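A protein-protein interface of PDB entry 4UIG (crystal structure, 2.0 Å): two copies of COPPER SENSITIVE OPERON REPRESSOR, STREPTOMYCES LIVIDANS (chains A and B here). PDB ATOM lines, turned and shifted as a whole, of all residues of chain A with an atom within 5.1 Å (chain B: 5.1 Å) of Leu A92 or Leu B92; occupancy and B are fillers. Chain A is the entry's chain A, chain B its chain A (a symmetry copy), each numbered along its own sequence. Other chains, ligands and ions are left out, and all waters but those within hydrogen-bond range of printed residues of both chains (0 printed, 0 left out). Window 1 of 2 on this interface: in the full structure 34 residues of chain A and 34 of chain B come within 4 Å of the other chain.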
ATOM      1  N   LEU A  58      26.168   5.991  29.292  1.00  0.00           N
ATOM      2  CA  LEU A  58      25.632   6.792  28.200  1.00  0.00           C
ATOM      3  C   LEU A  58      26.705   7.276  27.243  1.00  0.00           C
ATOM      4  O   LEU A  58      26.481   7.346  26.013  1.00  0.00           O
ATOM      5  CB  LEU A  58      24.794   7.981  28.708  1.00  0.00           C
ATOM      6  CG  LEU A  58      23.467   7.606  29.361  1.00  0.00           C
ATOM      7  CD1 LEU A  58      22.869   8.803  30.098  1.00  0.00           C
ATOM      8  CD2 LEU A  58      22.447   7.128  28.326  1.00  0.00           C
ATOM      9  N   ILE A  61      27.353   4.375  25.035  1.00  0.00           N
ATOM     10  CA  ILE A  61      26.293   4.278  24.022  1.00  0.00           C
ATOM     11  C   ILE A  61      26.469   5.343  22.935  1.00  0.00           C
ATOM     12  O   ILE A  61      26.336   5.067  21.714  1.00  0.00           O
ATOM     13  CB  ILE A  61      24.894   4.345  24.650  1.00  0.00           C
ATOM     14  CG1 ILE A  61      24.677   3.107  25.521  1.00  0.00           C
ATOM     15  CG2 ILE A  61      23.795   4.479  23.594  1.00  0.00           C
ATOM     16  CD1 ILE A  61      23.544   3.267  26.543  1.00  0.00           C
ATOM     17  N   ILE A  65      26.907   4.792  18.786  1.00  0.00           N
ATOM     18  CA  ILE A  65      26.157   5.429  17.711  1.00  0.00           C
ATOM     19  C   ILE A  65      27.121   6.075  16.687  1.00  0.00           C
ATOM     20  O   ILE A  65      26.870   6.045  15.481  1.00  0.00           O
ATOM     21  CB  ILE A  65      25.123   6.488  18.162  1.00  0.00           C
ATOM     22  CG1 ILE A  65      24.211   5.991  19.300  1.00  0.00           C
ATOM     23  CG2 ILE A  65      24.247   6.921  16.993  1.00  0.00           C
ATOM     24  CD1 ILE A  65      23.623   4.640  19.118  1.00  0.00           C
ATOM     25  N   LEU A  68      28.240   3.281  14.532  1.00  0.00           N
ATOM     26  CA  LEU A  68      27.261   2.968  13.503  1.00  0.00           C
ATOM     27  C   LEU A  68      27.367   3.875  12.305  1.00  0.00           C
ATOM     28  O   LEU A  68      27.205   3.430  11.158  1.00  0.00           O
ATOM     29  CB  LEU A  68      25.817   2.999  14.064  1.00  0.00           C
ATOM     30  CG  LEU A  68      25.443   1.867  15.006  1.00  0.00           C
ATOM     31  CD1 LEU A  68      24.100   2.238  15.662  1.00  0.00           C
ATOM     32  CD2 LEU A  68      25.327   0.546  14.230  1.00  0.00           C
ATOM     33  N   VAL A  85      23.635  -2.474  16.080  1.00  0.00           N
ATOM     34  CA  VAL A  85      22.361  -1.840  16.455  1.00  0.00           C
ATOM     35  C   VAL A  85      21.752  -2.571  17.694  1.00  0.00           C
ATOM     36  O   VAL A  85      21.361  -1.957  18.695  1.00  0.00           O
ATOM     37  CB  VAL A  85      21.339  -1.780  15.313  1.00  0.00           C
ATOM     38  CG1 VAL A  85      19.947  -1.271  15.790  1.00  0.00           C
ATOM     39  CG2 VAL A  85      21.808  -0.898  14.211  1.00  0.00           C
ATOM     40  N   SER A  88      23.586  -1.830  20.902  1.00  0.00           N
ATOM     41  CA  SER A  88      23.235  -0.490  21.357  1.00  0.00           C
ATOM     42  C   SER A  88      21.839  -0.473  21.996  1.00  0.00           C
ATOM     43  O   SER A  88      21.634   0.157  23.043  1.00  0.00           O
ATOM     44  CB  SER A  88      23.290   0.516  20.206  1.00  0.00           C
ATOM     45  OG  SER A  88      24.627   0.577  19.690  1.00  0.00           O
ATOM     46  N   THR A  89      20.886  -1.130  21.356  1.00  0.00           N
ATOM     47  CA  THR A  89      19.510  -1.179  21.902  1.00  0.00           C
ATOM     48  C   THR A  89      19.491  -1.918  23.243  1.00  0.00           C
ATOM     49  O   THR A  89      18.846  -1.499  24.204  1.00  0.00           O
ATOM     50  CB  THR A  89      18.533  -1.842  20.926  1.00  0.00           C
ATOM     51  OG1 THR A  89      19.100  -3.078  20.551  1.00  0.00           O
ATOM     52  CG2 THR A  89      18.322  -1.008  19.744  1.00  0.00           C
ATOM     53  N   LYS A  90      20.277  -2.973  23.323  1.00  0.00           N
ATOM     54  CA  LYS A  90      20.436  -3.681  24.534  1.00  0.00           C
ATOM     55  C   LYS A  90      21.133  -2.878  25.642  1.00  0.00           C
ATOM     56  O   LYS A  90      20.788  -3.037  26.812  1.00  0.00           O
ATOM     57  CB  LYS A  90      21.191  -4.963  24.258  1.00  0.00           C
ATOM     58  CG  LYS A  90      21.227  -5.948  25.393  1.00  0.00           C
ATOM     59  N   ALA A  91      22.151  -2.083  25.319  1.00  0.00           N
ATOM     60  CA  ALA A  91      22.788  -1.254  26.334  1.00  0.00           C
ATOM     61  C   ALA A  91      21.794  -0.194  26.873  1.00  0.00           C
ATOM     62  O   ALA A  91      21.822   0.105  28.071  1.00  0.00           O
ATOM     63  CB  ALA A  91      24.025  -0.580  25.788  1.00  0.00           C
ATOM     64  N   LEU A  92      20.970   0.353  25.991  1.00  0.00           N
ATOM     65  CA  LEU A  92      19.942   1.292  26.383  1.00  0.00           C
ATOM     66  C   LEU A  92      18.887   0.631  27.288  1.00  0.00           C
ATOM     67  O   LEU A  92      18.425   1.239  28.243  1.00  0.00           O
ATOM     68  CB  LEU A  92      19.281   1.897  25.198  1.00  0.00           C
ATOM     69  CG  LEU A  92      20.079   3.056  24.518  1.00  0.00           C
ATOM     70  CD1 LEU A  92      19.526   3.299  23.120  1.00  0.00           C
ATOM     71  CD2 LEU A  92      19.989   4.369  25.322  1.00  0.00           C
ATOM     72  N   GLN A  93      18.550  -0.622  26.994  1.00  0.00           N
ATOM     73  CA  GLN A  93      17.581  -1.365  27.795  1.00  0.00           C
ATOM     74  C   GLN A  93      18.093  -1.670  29.151  1.00  0.00           C
ATOM     75  O   GLN A  93      17.375  -1.619  30.138  1.00  0.00           O
ATOM     76  CB  GLN A  93      17.191  -2.651  27.091  1.00  0.00           C
ATOM     77  CG  GLN A  93      16.224  -2.389  25.984  1.00  0.00           C
ATOM     78  CD  GLN A  93      15.835  -3.649  25.229  1.00  0.00           C
ATOM     79  OE1 GLN A  93      15.957  -4.790  25.745  1.00  0.00           O
ATOM     80  NE2 GLN A  93      15.311  -3.458  24.025  1.00  0.00           N
ATOM     81  N   SER A  94      19.343  -2.026  29.205  1.00  0.00           N
ATOM     82  CA  SER A  94      19.996  -2.221  30.439  1.00  0.00           C
ATOM     83  C   SER A  94      20.103  -0.939  31.312  1.00  0.00           C
ATOM     84  O   SER A  94      19.898  -0.981  32.535  1.00  0.00           O
ATOM     85  CB  SER A  94      21.329  -2.867  30.185  1.00  0.00           C
ATOM     86  OG  SER A  94      22.027  -2.837  31.354  1.00  0.00           O
ATOM     87  N   PHE A  95      20.412   0.189  30.685  1.00  0.00           N
ATOM     88  CA  PHE A  95      20.333   1.493  31.355  1.00  0.00           C
ATOM     89  C   PHE A  95      18.895   1.771  31.890  1.00  0.00           C
ATOM     90  O   PHE A  95      18.761   2.166  33.045  1.00  0.00           O
ATOM     91  CB  PHE A  95      20.800   2.594  30.379  1.00  0.00           C
ATOM     92  CG  PHE A  95      20.569   3.996  30.867  1.00  0.00           C
ATOM     93  CD1 PHE A  95      21.302   4.504  31.929  1.00  0.00           C
ATOM     94  CD2 PHE A  95      19.636   4.816  30.248  1.00  0.00           C
ATOM     95  CE1 PHE A  95      21.108   5.821  32.360  1.00  0.00           C
ATOM     96  CE2 PHE A  95      19.421   6.134  30.684  1.00  0.00           C
ATOM     97  CZ  PHE A  95      20.160   6.628  31.743  1.00  0.00           C
ATOM     98  N   ALA A  96      17.869   1.511  31.080  1.00  0.00           N
ATOM     99  CA  ALA A  96      16.453   1.723  31.443  1.00  0.00           C
ATOM    100  C   ALA A  96      16.058   0.911  32.691  1.00  0.00           C
ATOM    101  O   ALA A  96      15.371   1.415  33.570  1.00  0.00           O
ATOM    102  CB  ALA A  96      15.540   1.377  30.296  1.00  0.00           C
ATOM    103  N   LEU B  58      20.858   8.469  12.131  1.00  0.00           N
ATOM    104  CA  LEU B  58      21.849   8.164  13.153  1.00  0.00           C
ATOM    105  C   LEU B  58      22.353   9.403  13.872  1.00  0.00           C
ATOM    106  O   LEU B  58      22.612   9.371  15.096  1.00  0.00           O
ATOM    107  CB  LEU B  58      23.033   7.354  12.593  1.00  0.00           C
ATOM    108  CG  LEU B  58      22.704   5.919  12.192  1.00  0.00           C
ATOM    109  CD1 LEU B  58      23.841   5.311  11.373  1.00  0.00           C
ATOM    110  CD2 LEU B  58      22.473   5.032  13.417  1.00  0.00           C
ATOM    111  N   ILE B  61      19.733  10.150  16.378  1.00  0.00           N
ATOM    112  CA  ILE B  61      19.879   9.249  17.530  1.00  0.00           C
ATOM    113  C   ILE B  61      21.061   9.667  18.411  1.00  0.00           C
ATOM    114  O   ILE B  61      20.969   9.697  19.667  1.00  0.00           O
ATOM    115  CB  ILE B  61      19.996   7.782  17.096  1.00  0.00           C
ATOM    116  CG1 ILE B  61      18.677   7.343  16.459  1.00  0.00           C
ATOM    117  CG2 ILE B  61      20.379   6.866  18.261  1.00  0.00           C
ATOM    118  CD1 ILE B  61      18.804   6.086  15.589  1.00  0.00           C
ATOM    119  N   ILE B  65      21.044  10.678  22.496  1.00  0.00           N
ATOM    120  CA  ILE B  65      21.892  10.148  23.557  1.00  0.00           C
ATOM    121  C   ILE B  65      22.576  11.300  24.330  1.00  0.00           C
ATOM    122  O   ILE B  65      22.735  11.231  25.551  1.00  0.00           O
ATOM    123  CB  ILE B  65      22.975   9.142  23.098  1.00  0.00           C
ATOM    124  CG1 ILE B  65      22.418   8.035  22.183  1.00  0.00           C
ATOM    125  CG2 ILE B  65      23.647   8.486  24.298  1.00  0.00           C
ATOM    126  CD1 ILE B  65      21.168   7.378  22.644  1.00  0.00           C
ATOM    127  N   LEU B  68      20.008  12.513  26.705  1.00  0.00           N
ATOM    128  CA  LEU B  68      19.935  11.677  27.893  1.00  0.00           C
ATOM    129  C   LEU B  68      20.983  12.030  28.916  1.00  0.00           C
ATOM    130  O   LEU B  68      20.717  12.009  30.129  1.00  0.00           O
ATOM    131  CB  LEU B  68      20.030  10.172  27.538  1.00  0.00           C
ATOM    132  CG  LEU B  68      18.821   9.576  26.836  1.00  0.00           C
ATOM    133  CD1 LEU B  68      19.227   8.183  26.322  1.00  0.00           C
ATOM    134  CD2 LEU B  68      17.636   9.477  27.809  1.00  0.00           C
ATOM    135  N   VAL B  85      14.570   7.302  26.681  1.00  0.00           N
ATOM    136  CA  VAL B  85      15.267   6.038  26.393  1.00  0.00           C
ATOM    137  C   VAL B  85      14.435   5.197  25.374  1.00  0.00           C
ATOM    138  O   VAL B  85      14.942   4.708  24.355  1.00  0.00           O
ATOM    139  CB  VAL B  85      15.582   5.206  27.643  1.00  0.00           C
ATOM    140  CG1 VAL B  85      16.154   3.801  27.291  1.00  0.00           C
ATOM    141  CG2 VAL B  85      16.557   5.901  28.526  1.00  0.00           C
ATOM    142  N   SER B  88      14.549   6.582  21.870  1.00  0.00           N
ATOM    143  CA  SER B  88      15.842   6.270  21.272  1.00  0.00           C
ATOM    144  C   SER B  88      15.906   4.799  20.835  1.00  0.00           C
ATOM    145  O   SER B  88      16.404   4.489  19.743  1.00  0.00           O
ATOM    146  CB  SER B  88      16.986   6.573  22.241  1.00  0.00           C
ATOM    147  OG  SER B  88      16.986   7.973  22.554  1.00  0.00           O
ATOM    148  N   THR B  89      15.439   3.905  21.691  1.00  0.00           N
ATOM    149  CA  THR B  89      15.449   2.463  21.351  1.00  0.00           C
ATOM    150  C   THR B  89      14.539   2.188  20.152  1.00  0.00           C
ATOM    151  O   THR B  89      14.883   1.440  19.236  1.00  0.00           O
ATOM    152  CB  THR B  89      15.024   1.595  22.540  1.00  0.00           C
ATOM    153  OG1 THR B  89      13.802   2.116  23.015  1.00  0.00           O
ATOM    154  CG2 THR B  89      16.029   1.628  23.602  1.00  0.00           C
ATOM    155  N   LYS B  90      13.412   2.870  20.124  1.00  0.00           N
ATOM    156  CA  LYS B  90      12.532   2.791  19.022  1.00  0.00           C
ATOM    157  C   LYS B  90      13.105   3.374  17.721  1.00  0.00           C
ATOM    158  O   LYS B  90      12.821   2.847  16.647  1.00  0.00           O
ATOM    159  CB  LYS B  90      11.233   3.479  19.381  1.00  0.00           C
ATOM    160  CG  LYS B  90      10.103   3.270  18.412  1.00  0.00           C
ATOM    161  N   ALA B  91      13.834   4.487  17.779  1.00  0.00           N
ATOM    162  CA  ALA B  91      14.450   5.026  16.574  1.00  0.00           C
ATOM    163  C   ALA B  91      15.517   4.046  16.024  1.00  0.00           C
ATOM    164  O   ALA B  91      15.645   3.917  14.803  1.00  0.00           O
ATOM    165  CB  ALA B  91      15.069   6.379  16.838  1.00  0.00           C
ATOM    166  N   LEU B  92      16.258   3.408  16.919  1.00  0.00           N
ATOM    167  CA  LEU B  92      17.229   2.408  16.535  1.00  0.00           C
ATOM    168  C   LEU B  92      16.556   1.182  15.893  1.00  0.00           C
ATOM    169  O   LEU B  92      17.069   0.630  14.930  1.00  0.00           O
ATOM    170  CB  LEU B  92      18.053   1.980  17.695  1.00  0.00           C
ATOM    171  CG  LEU B  92      19.211   2.957  18.079  1.00  0.00           C
ATOM    172  CD1 LEU B  92      19.696   2.639  19.487  1.00  0.00           C
ATOM    173  CD2 LEU B  92      20.404   2.847  17.107  1.00  0.00           C
ATOM    174  N   GLN B  93      15.394   0.798  16.414  1.00  0.00           N
ATOM    175  CA  GLN B  93      14.646  -0.334  15.873  1.00  0.00           C
ATOM    176  C   GLN B  93      14.110  -0.056  14.521  1.00  0.00           C
ATOM    177  O   GLN B  93      14.094  -0.907  13.645  1.00  0.00           O
ATOM    178  CB  GLN B  93      13.512  -0.711  16.809  1.00  0.00           C
ATOM    179  CG  GLN B  93      14.016  -1.479  17.986  1.00  0.00           C
ATOM    180  CD  GLN B  93      12.915  -1.846  18.967  1.00  0.00           C
ATOM    181  OE1 GLN B  93      11.709  -1.890  18.616  1.00  0.00           O
ATOM    182  NE2 GLN B  93      13.320  -2.168  20.189  1.00  0.00           N
ATOM    183  N   SER B  94      13.630   1.142  14.350  1.00  0.00           N
ATOM    184  CA  SER B  94      13.205   1.586  13.081  1.00  0.00           C
ATOM    185  C   SER B  94      14.339   1.659  12.021  1.00  0.00           C
ATOM    186  O   SER B  94      14.151   1.270  10.857  1.00  0.00           O
ATOM    187  CB  SER B  94      12.474   2.889  13.245  1.00  0.00           C
ATOM    188  OG  SER B  94      12.275   3.404  12.000  1.00  0.00           O
ATOM    189  N   PHE B  95      15.507   2.143  12.423  1.00  0.00           N
ATOM    190  CA  PHE B  95      16.708   2.064  11.582  1.00  0.00           C
ATOM    191  C   PHE B  95      17.048   0.588  11.215  1.00  0.00           C
ATOM    192  O   PHE B  95      17.293   0.314  10.043  1.00  0.00           O
ATOM    193  CB  PHE B  95      17.882   2.755  12.309  1.00  0.00           C
ATOM    194  CG  PHE B  95      19.220   2.561  11.654  1.00  0.00           C
ATOM    195  CD1 PHE B  95      19.504   3.164  10.438  1.00  0.00           C
ATOM    196  CD2 PHE B  95      20.204   1.797  12.266  1.00  0.00           C
ATOM    197  CE1 PHE B  95      20.762   3.009   9.845  1.00  0.00           C
ATOM    198  CE2 PHE B  95      21.464   1.621  11.670  1.00  0.00           C
ATOM    199  CZ  PHE B  95      21.734   2.228  10.458  1.00  0.00           C
ATOM    200  N   ALA B  96      17.003  -0.322  12.187  1.00  0.00           N
ATOM    201  CA  ALA B  96      17.300  -1.756  11.994  1.00  0.00           C
ATOM    202  C   ALA B  96      16.367  -2.394  10.948  1.00  0.00           C
ATOM    203  O   ALA B  96      16.810  -3.165  10.105  1.00  0.00           O
ATOM    204  CB  ALA B  96      17.205  -2.510  13.293  1.00  0.00           C
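The backbone carbonyl oxygen (O) of Val A85 lies within hydrogen-bond range of the side-chain hydroxyl (OG1) of Thr A89, at 3.1 Å. The backbone carbonyl oxygen (O) of Val B85 sits at hydrogen-bond distance from the side-chain hydroxyl (OG1) of Thr B89 (3.1 Å).
Val A85 touches Leu B92, and with the chains exchanged Leu A92 touches Val B85. Val A85 touches Phe B95, and with the chains exchanged Phe A95 touches Val B85. Thr A89 touches Leu B92, and with the chains exchanged Leu A92 touches Thr B89. Leu A92 touches its own counterpart, Leu B92. Positions printed for both chains: 58, 61, 65, 68, 85, 88, 89, 90, 91, 92, 93, 94, 95 and 96. Of the 14 pairs that touch across the chains among the printed residues, 14 have their exchanged pair printed and touching as well.
Of the 14 printed residues of chain A, 8 touch a printed residue of chain B. Printed residues of chain B that touch a printed residue of chain A: Leu B58, Ile B65, Leu B68, Val B85, Thr B89, Leu B92, Phe B95 and Ala B96. Among the printed residues, 14 pairs touch across the chains.
Of the printed residues of chain B, Leu A92 touches Val B85, Thr B89 and Leu B92. Printed residues of chain A within 4 Å of Leu B92: Val A85 (3.6 Å), Thr A89 (3.6 Å) and Leu A92 (3.7 Å). Printed residues of chain A within 4 Å of Ala B96: Val A85 (3.9 Å). Printed residues of chain B within 4 Å of Val A85: Leu B92, Phe B95 and Ala B96. Of the printed residues of chain A, Leu B58 touches Ile A65 (3.5 Å) and Leu A68 (3.9 Å). Printed residues of chain B within 4 Å of Ala A96: Val B85. Printed residues of chain B within 4 Å of Phe A95: Val B85. Gln B93 touches none of the printed residues of chain A. Ser A94 touches none of the printed residues of chain B. The nearest printed residue of chain B that does not touch Phe A95 is Leu B68 (4.8 Å).
Among the printed residues, pairs that only touch across the chains: Leu A58 with Ile B65 (3.5 Å), Ile A65 with Leu B58 (3.5 Å), Leu A92 with Val B85 (3.6 Å), Val A85 with Leu B92 (3.6 Å), Phe A95 with Val B85 (3.6 Å), Val A85 with Phe B95 (3.6 Å), Leu A92 with Thr B89 (3.6 Å), Thr A89 with Leu B92 (3.6 Å), Leu A92 with Leu B92 (3.7 Å), Leu A68 with Leu B58 (3.9 Å), Leu A58 with Leu B68 (3.9 Å), Ala A96 with Val B85 (3.9 Å), Val A85 with Ala B96 (3.9 Å) and Ile A65 with Ile B65 (3.96 Å).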
